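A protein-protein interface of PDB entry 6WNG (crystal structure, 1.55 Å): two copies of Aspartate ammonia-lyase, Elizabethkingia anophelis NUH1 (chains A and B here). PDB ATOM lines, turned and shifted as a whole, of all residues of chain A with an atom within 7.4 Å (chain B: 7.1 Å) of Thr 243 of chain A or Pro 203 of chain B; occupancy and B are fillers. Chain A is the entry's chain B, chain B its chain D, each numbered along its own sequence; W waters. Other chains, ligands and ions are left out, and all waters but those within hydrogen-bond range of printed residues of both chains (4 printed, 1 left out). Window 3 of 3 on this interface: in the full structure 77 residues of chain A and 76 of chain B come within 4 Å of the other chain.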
ATOM      1  N   GLY A 237       7.748 -39.447  24.798  1.00  0.00           N
ATOM      2  CA  GLY A 237       7.647 -38.012  24.944  1.00  0.00           C
ATOM      3  C   GLY A 237       8.391 -37.236  23.879  1.00  0.00           C
ATOM      4  O   GLY A 237       8.197 -36.019  23.778  1.00  0.00           O
ATOM      5  N   ALA A 238       9.239 -37.903  23.083  1.00  0.00           N
ATOM      6  CA  ALA A 238       9.900 -37.231  21.971  1.00  0.00           C
ATOM      7  C   ALA A 238       8.906 -36.727  20.931  1.00  0.00           C
ATOM      8  O   ALA A 238       9.173 -35.730  20.249  1.00  0.00           O
ATOM      9  CB  ALA A 238      10.889 -38.189  21.299  1.00  0.00           C
ATOM     10  N   THR A 239       7.758 -37.397  20.808  1.00  0.00           N
ATOM     11  CA  THR A 239       6.829 -37.281  19.686  1.00  0.00           C
ATOM     12  C   THR A 239       7.611 -37.257  18.367  1.00  0.00           C
ATOM     13  O   THR A 239       8.442 -38.144  18.157  1.00  0.00           O
ATOM     14  CB  THR A 239       5.838 -36.102  19.879  1.00  0.00           C
ATOM     15  OG1 THR A 239       6.447 -34.816  19.670  1.00  0.00           O
ATOM     16  CG2 THR A 239       5.222 -36.142  21.284  1.00  0.00           C
ATOM     17  N   ALA A 240       7.358 -36.295  17.470  1.00  0.00           N
ATOM     18  CA  ALA A 240       7.774 -36.449  16.070  1.00  0.00           C
ATOM     19  C   ALA A 240       9.296 -36.494  15.901  1.00  0.00           C
ATOM     20  O   ALA A 240       9.818 -37.329  15.146  1.00  0.00           O
ATOM     21  CB  ALA A 240       7.169 -35.325  15.219  1.00  0.00           C
ATOM     22  N   ILE A 241      10.029 -35.570  16.531  1.00  0.00           N
ATOM     23  CA  ILE A 241      11.464 -35.454  16.290  1.00  0.00           C
ATOM     24  C   ILE A 241      12.285 -35.320  17.563  1.00  0.00           C
ATOM     25  O   ILE A 241      13.509 -35.206  17.477  1.00  0.00           O
ATOM     26  CB  ILE A 241      11.794 -34.282  15.339  1.00  0.00           C
ATOM     27  CG1 ILE A 241      11.391 -32.943  15.963  1.00  0.00           C
ATOM     28  CG2 ILE A 241      11.120 -34.470  13.975  1.00  0.00           C
ATOM     29  CD1 ILE A 241      11.866 -31.723  15.151  1.00  0.00           C
ATOM     30  N   GLY A 242      11.662 -35.308  18.740  1.00  0.00           N
ATOM     31  CA  GLY A 242      12.370 -35.120  19.992  1.00  0.00           C
ATOM     32  C   GLY A 242      12.044 -33.826  20.709  1.00  0.00           C
ATOM     33  O   GLY A 242      12.449 -33.662  21.871  1.00  0.00           O
ATOM     34  N   THR A 243      11.331 -32.899  20.066  1.00  0.00           N
ATOM     35  CA  THR A 243      10.968 -31.646  20.719  1.00  0.00           C
ATOM     36  C   THR A 243       9.824 -31.795  21.709  1.00  0.00           C
ATOM     37  O   THR A 243       9.588 -30.877  22.505  1.00  0.00           O
ATOM     38  CB  THR A 243      10.563 -30.594  19.690  1.00  0.00           C
ATOM     39  OG1 THR A 243       9.485 -31.108  18.892  1.00  0.00           O
ATOM     40  CG2 THR A 243      11.747 -30.241  18.804  1.00  0.00           C
ATOM     41  N   GLY A 244       9.085 -32.899  21.661  1.00  0.00           N
ATOM     42  CA  GLY A 244       7.947 -33.052  22.545  1.00  0.00           C
ATOM     43  C   GLY A 244       6.720 -32.270  22.138  1.00  0.00           C
ATOM     44  O   GLY A 244       5.797 -32.137  22.948  1.00  0.00           O
ATOM     45  N   LEU A 245       6.678 -31.761  20.905  1.00  0.00           N
ATOM     46  CA  LEU A 245       5.503 -31.051  20.417  1.00  0.00           C
ATOM     47  C   LEU A 245       4.258 -31.906  20.620  1.00  0.00           C
ATOM     48  O   LEU A 245       4.245 -33.094  20.278  1.00  0.00           O
ATOM     49  CB  LEU A 245       5.684 -30.711  18.937  1.00  0.00           C
ATOM     50  CG  LEU A 245       4.525 -29.943  18.303  1.00  0.00           C
ATOM     51  CD1 LEU A 245       4.442 -28.522  18.862  1.00  0.00           C
ATOM     52  CD2 LEU A 245       4.630 -29.937  16.773  1.00  0.00           C
ATOM     53  N   ASN A 246       3.233 -31.300  21.220  1.00  0.00           N
ATOM     54  CA  ASN A 246       1.922 -31.868  21.539  1.00  0.00           C
ATOM     55  C   ASN A 246       1.929 -32.739  22.799  1.00  0.00           C
ATOM     56  O   ASN A 246       0.856 -33.187  23.205  1.00  0.00           O
ATOM     57  CB  ASN A 246       1.315 -32.670  20.375  1.00  0.00           C
ATOM     58  CG  ASN A 246       0.977 -31.786  19.197  1.00  0.00           C
ATOM     59  OD1 ASN A 246       1.065 -30.561  19.297  1.00  0.00           O
ATOM     60  ND2 ASN A 246       0.589 -32.393  18.082  1.00  0.00           N
ATOM     61  N   ALA A 247       3.071 -32.964  23.446  1.00  0.00           N
ATOM     62  CA  ALA A 247       3.075 -33.659  24.728  1.00  0.00           C
ATOM     63  C   ALA A 247       2.980 -32.670  25.887  1.00  0.00           C
ATOM     64  O   ALA A 247       3.447 -31.533  25.804  1.00  0.00           O
ATOM     65  CB  ALA A 247       4.333 -34.522  24.884  1.00  0.00           C
ATOM     66  N   LEU A 273      15.970 -35.993  24.099  1.00  0.00           N
ATOM     67  CA  LEU A 273      15.066 -36.701  23.200  1.00  0.00           C
ATOM     68  C   LEU A 273      15.323 -36.364  21.738  1.00  0.00           C
ATOM     69  O   LEU A 273      15.005 -37.174  20.859  1.00  0.00           O
ATOM     70  CB  LEU A 273      13.612 -36.400  23.569  1.00  0.00           C
ATOM     71  CG  LEU A 273      13.237 -36.806  24.998  1.00  0.00           C
ATOM     72  CD1 LEU A 273      11.776 -36.470  25.288  1.00  0.00           C
ATOM     73  CD2 LEU A 273      13.498 -38.294  25.210  1.00  0.00           C
ATOM     74  N   VAL A 274      15.914 -35.199  21.455  1.00  0.00           N
ATOM     75  CA  VAL A 274      16.309 -34.892  20.083  1.00  0.00           C
ATOM     76  C   VAL A 274      17.468 -35.794  19.657  1.00  0.00           C
ATOM     77  O   VAL A 274      17.505 -36.311  18.531  1.00  0.00           O
ATOM     78  CB  VAL A 274      16.663 -33.395  19.961  1.00  0.00           C
ATOM     79  CG1 VAL A 274      17.201 -33.072  18.568  1.00  0.00           C
ATOM     80  CG2 VAL A 274      15.452 -32.502  20.302  1.00  0.00           C
ATOM     81  N   THR A 277      16.048 -39.633  19.148  1.00  0.00           N
ATOM     82  CA  THR A 277      15.072 -40.034  18.139  1.00  0.00           C
ATOM     83  C   THR A 277      15.731 -40.607  16.877  1.00  0.00           C
ATOM     84  O   THR A 277      15.238 -41.620  16.364  1.00  0.00           O
ATOM     85  CB  THR A 277      14.126 -38.856  17.855  1.00  0.00           C
ATOM     86  OG1 THR A 277      13.405 -38.566  19.066  1.00  0.00           O
ATOM     87  CG2 THR A 277      13.115 -39.193  16.751  1.00  0.00           C
ATOM     88  N   ILE B 191      15.857 -21.010  14.408  1.00  0.00           N
ATOM     89  CA  ILE B 191      14.710 -21.894  14.243  1.00  0.00           C
ATOM     90  C   ILE B 191      14.687 -22.408  12.811  1.00  0.00           C
ATOM     91  O   ILE B 191      14.907 -21.652  11.855  1.00  0.00           O
ATOM     92  CB  ILE B 191      13.408 -21.163  14.614  1.00  0.00           C
ATOM     93  CG1 ILE B 191      13.494 -20.671  16.060  1.00  0.00           C
ATOM     94  CG2 ILE B 191      12.221 -22.103  14.465  1.00  0.00           C
ATOM     95  CD1 ILE B 191      12.312 -19.831  16.515  1.00  0.00           C
ATOM     96  N   LYS B 192      14.435 -23.709  12.663  1.00  0.00           N
ATOM     97  CA  LYS B 192      14.537 -24.377  11.373  1.00  0.00           C
ATOM     98  C   LYS B 192      13.528 -25.518  11.318  1.00  0.00           C
ATOM     99  O   LYS B 192      12.889 -25.856  12.318  1.00  0.00           O
ATOM    100  CB  LYS B 192      15.956 -24.913  11.145  1.00  0.00           C
ATOM    101  CG  LYS B 192      16.449 -25.816  12.268  1.00  0.00           C
ATOM    102  CD  LYS B 192      17.537 -26.776  11.789  1.00  0.00           C
ATOM    103  CE  LYS B 192      16.956 -27.912  10.956  1.00  0.00           C
ATOM    104  NZ  LYS B 192      18.025 -28.684  10.241  1.00  0.00           N
ATOM    105  N   MET B 193      13.400 -26.137  10.145  1.00  0.00           N
ATOM    106  CA  MET B 193      12.471 -27.255   9.991  1.00  0.00           C
ATOM    107  C   MET B 193      13.191 -28.580  10.217  1.00  0.00           C
ATOM    108  O   MET B 193      14.157 -28.902   9.516  1.00  0.00           O
ATOM    109  CB  MET B 193      11.808 -27.267   8.612  1.00  0.00           C
ATOM    110  CG  MET B 193      10.646 -26.292   8.468  1.00  0.00           C
ATOM    111  SD  MET B 193       9.341 -26.587   9.694  1.00  0.00           S
ATOM    112  CE  MET B 193       8.632 -28.137   9.157  1.00  0.00           C
ATOM    113  N   GLY B 194      12.715 -29.347  11.190  1.00  0.00           N
ATOM    114  CA  GLY B 194      13.080 -30.743  11.241  1.00  0.00           C
ATOM    115  C   GLY B 194      12.545 -31.498  10.039  1.00  0.00           C
ATOM    116  O   GLY B 194      11.564 -31.104   9.401  1.00  0.00           O
ATOM    117  N   ALA B 201       8.992 -32.027   8.641  1.00  0.00           N
ATOM    118  CA  ALA B 201       8.408 -32.552   9.872  1.00  0.00           C
ATOM    119  C   ALA B 201       7.801 -31.425  10.713  1.00  0.00           C
ATOM    120  O   ALA B 201       6.716 -30.930  10.388  1.00  0.00           O
ATOM    121  CB  ALA B 201       9.457 -33.346  10.661  1.00  0.00           C
ATOM    122  N   VAL B 202       8.463 -31.036  11.805  1.00  0.00           N
ATOM    123  CA  VAL B 202       8.014 -29.955  12.692  1.00  0.00           C
ATOM    124  C   VAL B 202       9.219 -29.087  13.053  1.00  0.00           C
ATOM    125  O   VAL B 202      10.360 -29.493  12.772  1.00  0.00           O
ATOM    126  CB  VAL B 202       7.321 -30.515  13.949  1.00  0.00           C
ATOM    127  CG1 VAL B 202       6.009 -31.217  13.572  1.00  0.00           C
ATOM    128  CG2 VAL B 202       8.261 -31.440  14.720  1.00  0.00           C
ATOM    129  N   PRO B 203       9.033 -27.895  13.633  1.00  0.00           N
ATOM    130  CA  PRO B 203      10.181 -27.018  13.905  1.00  0.00           C
ATOM    131  C   PRO B 203      11.108 -27.545  14.992  1.00  0.00           C
ATOM    132  O   PRO B 203      10.731 -28.330  15.867  1.00  0.00           O
ATOM    133  CB  PRO B 203       9.528 -25.699  14.344  1.00  0.00           C
ATOM    134  CG  PRO B 203       8.132 -25.739  13.739  1.00  0.00           C
ATOM    135  CD  PRO B 203       7.754 -27.197  13.861  1.00  0.00           C
ATOM    136  N   MET B 204      12.355 -27.083  14.919  1.00  0.00           N
ATOM    137  CA  MET B 204      13.354 -27.306  15.960  1.00  0.00           C
ATOM    138  C   MET B 204      14.317 -26.124  15.914  1.00  0.00           C
ATOM    139  O   MET B 204      14.197 -25.247  15.059  1.00  0.00           O
ATOM    140  CB  MET B 204      14.076 -28.640  15.759  1.00  0.00           C
ATOM    141  CG  MET B 204      14.950 -28.672  14.502  1.00  0.00           C
ATOM    142  SD  MET B 204      15.662 -30.288  14.133  1.00  0.00           S
ATOM    143  CE  MET B 204      16.470 -30.651  15.699  1.00  0.00           C
ATOM    144  N   THR B 205      15.280 -26.090  16.826  1.00  0.00           N
ATOM    145  CA  THR B 205      16.360 -25.126  16.670  1.00  0.00           C
ATOM    146  C   THR B 205      17.620 -25.845  16.223  1.00  0.00           C
ATOM    147  O   THR B 205      17.800 -27.044  16.468  1.00  0.00           O
ATOM    148  CB  THR B 205      16.663 -24.333  17.948  1.00  0.00           C
ATOM    149  OG1 THR B 205      17.319 -25.180  18.899  1.00  0.00           O
ATOM    150  CG2 THR B 205      15.389 -23.745  18.542  1.00  0.00           C
ATOM    151  N   GLN B 208      19.316 -27.265  19.200  1.00  0.00           N
ATOM    152  CA  GLN B 208      18.903 -28.629  19.524  1.00  0.00           C
ATOM    153  C   GLN B 208      19.619 -29.646  18.644  1.00  0.00           C
ATOM    154  O   GLN B 208      20.078 -30.687  19.131  1.00  0.00           O
ATOM    155  CB  GLN B 208      17.385 -28.771  19.373  1.00  0.00           C
ATOM    156  CG  GLN B 208      16.601 -28.111  20.497  1.00  0.00           C
ATOM    157  CD  GLN B 208      15.116 -28.000  20.192  1.00  0.00           C
ATOM    158  OE1 GLN B 208      14.722 -27.739  19.050  1.00  0.00           O
ATOM    159  NE2 GLN B 208      14.283 -28.199  21.211  1.00  0.00           N
ATOM    160  N   VAL B 411      10.257 -22.465   8.089  1.00  0.00           N
ATOM    161  CA  VAL B 411       9.295 -22.770   9.140  1.00  0.00           C
ATOM    162  C   VAL B 411       8.004 -21.990   8.919  1.00  0.00           C
ATOM    163  O   VAL B 411       6.906 -22.557   8.949  1.00  0.00           O
ATOM    164  CB  VAL B 411       9.902 -22.472  10.525  1.00  0.00           C
ATOM    165  CG1 VAL B 411       8.840 -22.596  11.615  1.00  0.00           C
ATOM    166  CG2 VAL B 411      11.083 -23.395  10.798  1.00  0.00           C
ATOM    167  N   SER B 414       5.901 -23.379   6.101  1.00  0.00           N
ATOM    168  CA  SER B 414       5.687 -24.814   6.068  1.00  0.00           C
ATOM    169  C   SER B 414       4.220 -25.164   6.291  1.00  0.00           C
ATOM    170  O   SER B 414       3.425 -24.374   6.820  1.00  0.00           O
ATOM    171  CB  SER B 414       6.533 -25.510   7.130  1.00  0.00           C
ATOM    172  OG  SER B 414       5.986 -25.257   8.402  1.00  0.00           O
ATOM    173  N   GLY B 416       3.933 -28.225   7.895  1.00  0.00           N
ATOM    174  CA  GLY B 416       4.133 -29.097   9.040  1.00  0.00           C
ATOM    175  C   GLY B 416       3.788 -28.483  10.380  1.00  0.00           C
ATOM    176  O   GLY B 416       3.513 -29.218  11.333  1.00  0.00           O
ATOM    177  N   ILE B 417       3.793 -27.152  10.485  1.00  0.00           N
ATOM    178  CA  ILE B 417       3.348 -26.514  11.718  1.00  0.00           C
ATOM    179  C   ILE B 417       1.889 -26.822  12.040  1.00  0.00           C
ATOM    180  O   ILE B 417       1.459 -26.610  13.179  1.00  0.00           O
ATOM    181  CB  ILE B 417       3.583 -24.986  11.655  1.00  0.00           C
ATOM    182  CG1 ILE B 417       2.954 -24.381  10.394  1.00  0.00           C
ATOM    183  CG2 ILE B 417       5.072 -24.685  11.723  1.00  0.00           C
ATOM    184  CD1 ILE B 417       3.036 -22.863  10.337  1.00  0.00           C
ATOM    185  N   THR B 419       0.764 -29.557  12.597  1.00  0.00           N
ATOM    186  CA  THR B 419       0.812 -30.583  13.635  1.00  0.00           C
ATOM    187  C   THR B 419       0.437 -30.014  15.001  1.00  0.00           C
ATOM    188  O   THR B 419      -0.235 -30.675  15.806  1.00  0.00           O
ATOM    189  CB  THR B 419       2.218 -31.190  13.679  1.00  0.00           C
ATOM    190  OG1 THR B 419       2.587 -31.647  12.371  1.00  0.00           O
ATOM    191  CG2 THR B 419       2.290 -32.363  14.657  1.00  0.00           C
ATOM    192  N   ALA B 420       0.853 -28.774  15.272  1.00  0.00           N
ATOM    193  CA  ALA B 420       0.579 -28.131  16.553  1.00  0.00           C
ATOM    194  C   ALA B 420      -0.913 -27.942  16.830  1.00  0.00           C
ATOM    195  O   ALA B 420      -1.283 -27.670  17.981  1.00  0.00           O
ATOM    196  CB  ALA B 420       1.297 -26.779  16.603  1.00  0.00           C
ATOM    197  N   ALA B 464       3.018 -20.054  16.922  1.00  0.00           N
ATOM    198  CA  ALA B 464       4.262 -19.310  17.049  1.00  0.00           C
ATOM    199  C   ALA B 464       5.418 -20.300  17.051  1.00  0.00           C
ATOM    200  O   ALA B 464       5.399 -21.257  17.834  1.00  0.00           O
ATOM    201  CB  ALA B 464       4.277 -18.470  18.321  1.00  0.00           C
ATOM    202  N   PRO B 465       6.416 -20.130  16.176  1.00  0.00           N
ATOM    203  CA  PRO B 465       7.491 -21.136  16.095  1.00  0.00           C
ATOM    204  C   PRO B 465       8.212 -21.349  17.414  1.00  0.00           C
ATOM    205  O   PRO B 465       8.548 -22.490  17.756  1.00  0.00           O
ATOM    206  CB  PRO B 465       8.425 -20.559  15.018  1.00  0.00           C
ATOM    207  CG  PRO B 465       7.565 -19.635  14.215  1.00  0.00           C
ATOM    208  CD  PRO B 465       6.588 -19.047  15.195  1.00  0.00           C
ATOM    209  N   GLU B 466       8.439 -20.277  18.177  1.00  0.00           N
ATOM    210  CA  GLU B 466       9.106 -20.407  19.464  1.00  0.00           C
ATOM    211  C   GLU B 466       8.295 -21.218  20.468  1.00  0.00           C
ATOM    212  O   GLU B 466       8.855 -21.637  21.487  1.00  0.00           O
ATOM    213  CB  GLU B 466       9.417 -19.023  20.038  1.00  0.00           C
ATOM    214  CG  GLU B 466       8.193 -18.187  20.365  1.00  0.00           C
ATOM    215  CD  GLU B 466       7.888 -17.139  19.308  1.00  0.00           C
ATOM    216  OE1 GLU B 466       8.213 -17.367  18.120  1.00  0.00           O
ATOM    217  OE2 GLU B 466       7.325 -16.081  19.670  1.00  0.00           O
ATOM    218  N   MET B 468       6.837 -24.154  19.683  1.00  0.00           N
ATOM    219  CA  MET B 468       6.764 -25.532  19.214  1.00  0.00           C
ATOM    220  C   MET B 468       8.013 -26.331  19.527  1.00  0.00           C
ATOM    221  O   MET B 468       8.162 -27.461  19.044  1.00  0.00           O
ATOM    222  CB  MET B 468       6.520 -25.562  17.715  1.00  0.00           C
ATOM    223  CG  MET B 468       5.243 -24.939  17.324  1.00  0.00           C
ATOM    224  SD  MET B 468       4.885 -25.543  15.688  1.00  0.00           S
ATOM    225  CE  MET B 468       3.942 -24.174  15.132  1.00  0.00           C
ATOM    226  N   LEU B 469       8.912 -25.773  20.316  1.00  0.00           N
ATOM    227  CA  LEU B 469      10.228 -26.344  20.524  1.00  0.00           C
ATOM    228  C   LEU B 469      10.306 -27.207  21.773  1.00  0.00           C
ATOM    229  O   LEU B 469      11.339 -27.848  21.999  1.00  0.00           O
ATOM    230  CB  LEU B 469      11.259 -25.207  20.593  1.00  0.00           C
ATOM    231  CG  LEU B 469      11.148 -24.229  19.415  1.00  0.00           C
ATOM    232  CD1 LEU B 469      12.006 -22.999  19.650  1.00  0.00           C
ATOM    233  CD2 LEU B 469      11.548 -24.909  18.110  1.00  0.00           C
ATOM    234  N   ASN B 470       9.235 -27.257  22.560  1.00  0.00           N
ATOM    235  CA  ASN B 470       9.191 -27.942  23.843  1.00  0.00           C
ATOM    236  C   ASN B 470       7.776 -28.442  24.070  1.00  0.00           C
ATOM    237  O   ASN B 470       6.830 -27.954  23.438  1.00  0.00           O
ATOM    238  CB  ASN B 470       9.583 -27.011  25.001  1.00  0.00           C
ATOM    239  CG  ASN B 470      10.836 -26.230  24.729  1.00  0.00           C
ATOM    240  OD1 ASN B 470      11.928 -26.624  25.135  1.00  0.00           O
ATOM    241  ND2 ASN B 470      10.690 -25.108  24.031  1.00  0.00           N
ATOM    242  N   PRO B 471       7.587 -29.384  24.988  1.00  0.00           N
ATOM    243  CA  PRO B 471       6.231 -29.695  25.440  1.00  0.00           C
ATOM    244  C   PRO B 471       5.656 -28.524  26.222  1.00  0.00           C
ATOM    245  O   PRO B 471       6.379 -27.758  26.863  1.00  0.00           O
ATOM    246  CB  PRO B 471       6.422 -30.928  26.333  1.00  0.00           C
ATOM    247  CG  PRO B 471       7.851 -30.894  26.743  1.00  0.00           C
ATOM    248  CD  PRO B 471       8.605 -30.240  25.627  1.00  0.00           C
ATOM    249  N   HIS B 472       4.329 -28.397  26.151  1.00  0.00           N
ATOM    250  CA  HIS B 472       3.598 -27.291  26.756  1.00  0.00           C
ATOM    251  C   HIS B 472       2.228 -27.779  27.208  1.00  0.00           C
ATOM    252  O   HIS B 472       1.706 -28.775  26.702  1.00  0.00           O
ATOM    253  CB  HIS B 472       3.410 -26.122  25.777  1.00  0.00           C
ATOM    254  CG  HIS B 472       4.683 -25.453  25.365  1.00  0.00           C
ATOM    255  ND1 HIS B 472       5.451 -24.713  26.239  1.00  0.00           N
ATOM    256  CD2 HIS B 472       5.312 -25.392  24.167  1.00  0.00           C
ATOM    257  CE1 HIS B 472       6.506 -24.237  25.600  1.00  0.00           C
ATOM    258  NE2 HIS B 472       6.444 -24.633  24.342  1.00  0.00           N
HETATM  259  O   HOH W   1       2.485 -29.612  23.859  1.00  0.00           O
HETATM  260  O   HOH W   2       8.582 -29.234  17.183  1.00  0.00           O
HETATM  261  O   HOH W   3       0.303 -28.091  20.200  1.00  0.00           O
HETATM  262  O   HOH W   4       4.145 -28.459  22.409  1.00  0.00           O
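No residue of chain B comes within 4 Å of Gly 242 of chain A. Of chain B, only Pro 203, Gln 208, Met 468, Leu 469, Asn 470 and Pro 471 come within 4 Å of Thr 243 of chain A. Pro 203 of chain B touches just these residues of chain A: Ile 241 and Thr 243. Of the printed residues of chain A, Gln 208 of chain B touches Thr 243 and Val 274. Ser 414 of chain B touches none of the printed residues of chain A. Of the printed residues of chain A, Leu 469 of chain B touches Thr 243 (3.5 Å). The nearest residue of chain B that does not touch Thr 243 of chain A is Met 204 of chain B (4.2 Å). The nearest printed residue of chain B that does not touch Val 274 of chain A is Thr 205 of chain B (6.4 Å).
Water W2 lies within hydrogen-bond range of the backbone carbonyl oxygen (O) of Met 468 of chain B, the backbone carbonyl oxygen (O) of Pro 203 of chain B and the side-chain hydroxyl (OG1) of Thr 243 of chain A. Water W3 bridges OD1 of Asn 246 of chain A and O of Ala 420 of chain B. Water W1 lies within hydrogen-bond range of O of Ala 247 of chain A (2.9 Å), O of His 472 of chain B (3.1 Å) and N of Asn 246 of chain A (3.2 Å). Water W4 bridges O of Asn 470 of chain B (2.9 Å) and N of Asn 246 of chain A (3.2 Å).
Among the printed residues, merely in contact across the chains: Ile 241 of chain A with Ala 201 of chain B, Ile 241 of chain A with Val 202 of chain B, Ile 241 of chain A with Pro 203 of chain B, Ile 241 of chain A with Met 204 of chain B, Thr 243 of chain A with Pro 203 of chain B, Thr 243 of chain A with Gln 208 of chain B, Thr 243 of chain A with Met 468 of chain B, Thr 243 of chain A with Leu 469 of chain B, Thr 243 of chain A with Asn 470 of chain B, Thr 243 of chain A with Pro 471 of chain B, Gly 244 of chain A with Pro 471 of chain B, Leu 245 of chain A with Val 202 of chain B, Leu 245 of chain A with Thr 419 of chain B, Leu 245 of chain A with Met 468 of chain B, Asn 246 of chain A with Ala 420 of chain B, Ala 247 of chain A with Pro 471 of chain B, Val 274 of chain A with Met 204 of chain B and Val 274 of chain A with Gln 208 of chain B.
The backbone carbonyl oxygen (O) of Ala 238 of chain A is in hydrogen-bond range of the backbone NH (N) of Gly 244 of chain A, 3.2 Å away. The backbone carbonyl oxygen (O) of Met 204 of chain B lies within hydrogen-bond range of the backbone NH (N) of Lys 192 of chain B (2.9 Å). The backbone carbonyl oxygen (O) of Gly 194 of chain B lies within hydrogen-bond range of the backbone NH (N) of Ala 201 of chain B, 2.8 Å away. The side-chain amide oxygen of Gln 208 of chain B is in hydrogen-bond range of the backbone NH of Thr 205 of chain B (2.8 Å). NE2 of Gln 208 of chain B lies within hydrogen-bond range of O of Leu 469 of chain B (3.1 Å). The backbone carbonyl oxygen of Gly 416 of chain B is in hydrogen-bond range of the side-chain hydroxyl of Thr 419 of chain B.
No position is printed for both chains. Of the 20 pairs that touch across the chains among the printed residues, none has its exchanged pair printed and touching as well.
Of the 24 printed residues of chain B, 12 touch a printed residue of chain A. Printed residues of chain B that touch a printed residue of chain A: Ala 201, Val 202, Pro 203, Met 204, Gln 208, Thr 419, Ala 420, Met 468, Leu 469, Asn 470, Pro 471 and His 472. Hydrophobic or aromatic side chains of chain B within 4 Å of the printed part of chain A: Ala 201, Val 202, Met 204, Met 468 and Pro 471. Hydrophobic or aromatic side chains of chain A that line the printed part of chain B: Ile 241, Leu 245 and Val 274. Among the printed residues, 20 pairs touch across the chains. Among the printed residues, no Asp or Glu carboxylate lies within 4 Å of a Lys or Arg side-chain nitrogen of the other chain.
The side-chain amide nitrogen (ND2) of Asn 246 of chain A sits at hydrogen-bond distance from the backbone carbonyl oxygen (O) of Thr 419 of chain B. O of Ala 247 of chain A sits at hydrogen-bond distance from N of His 472 of chain B (3.3 Å).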
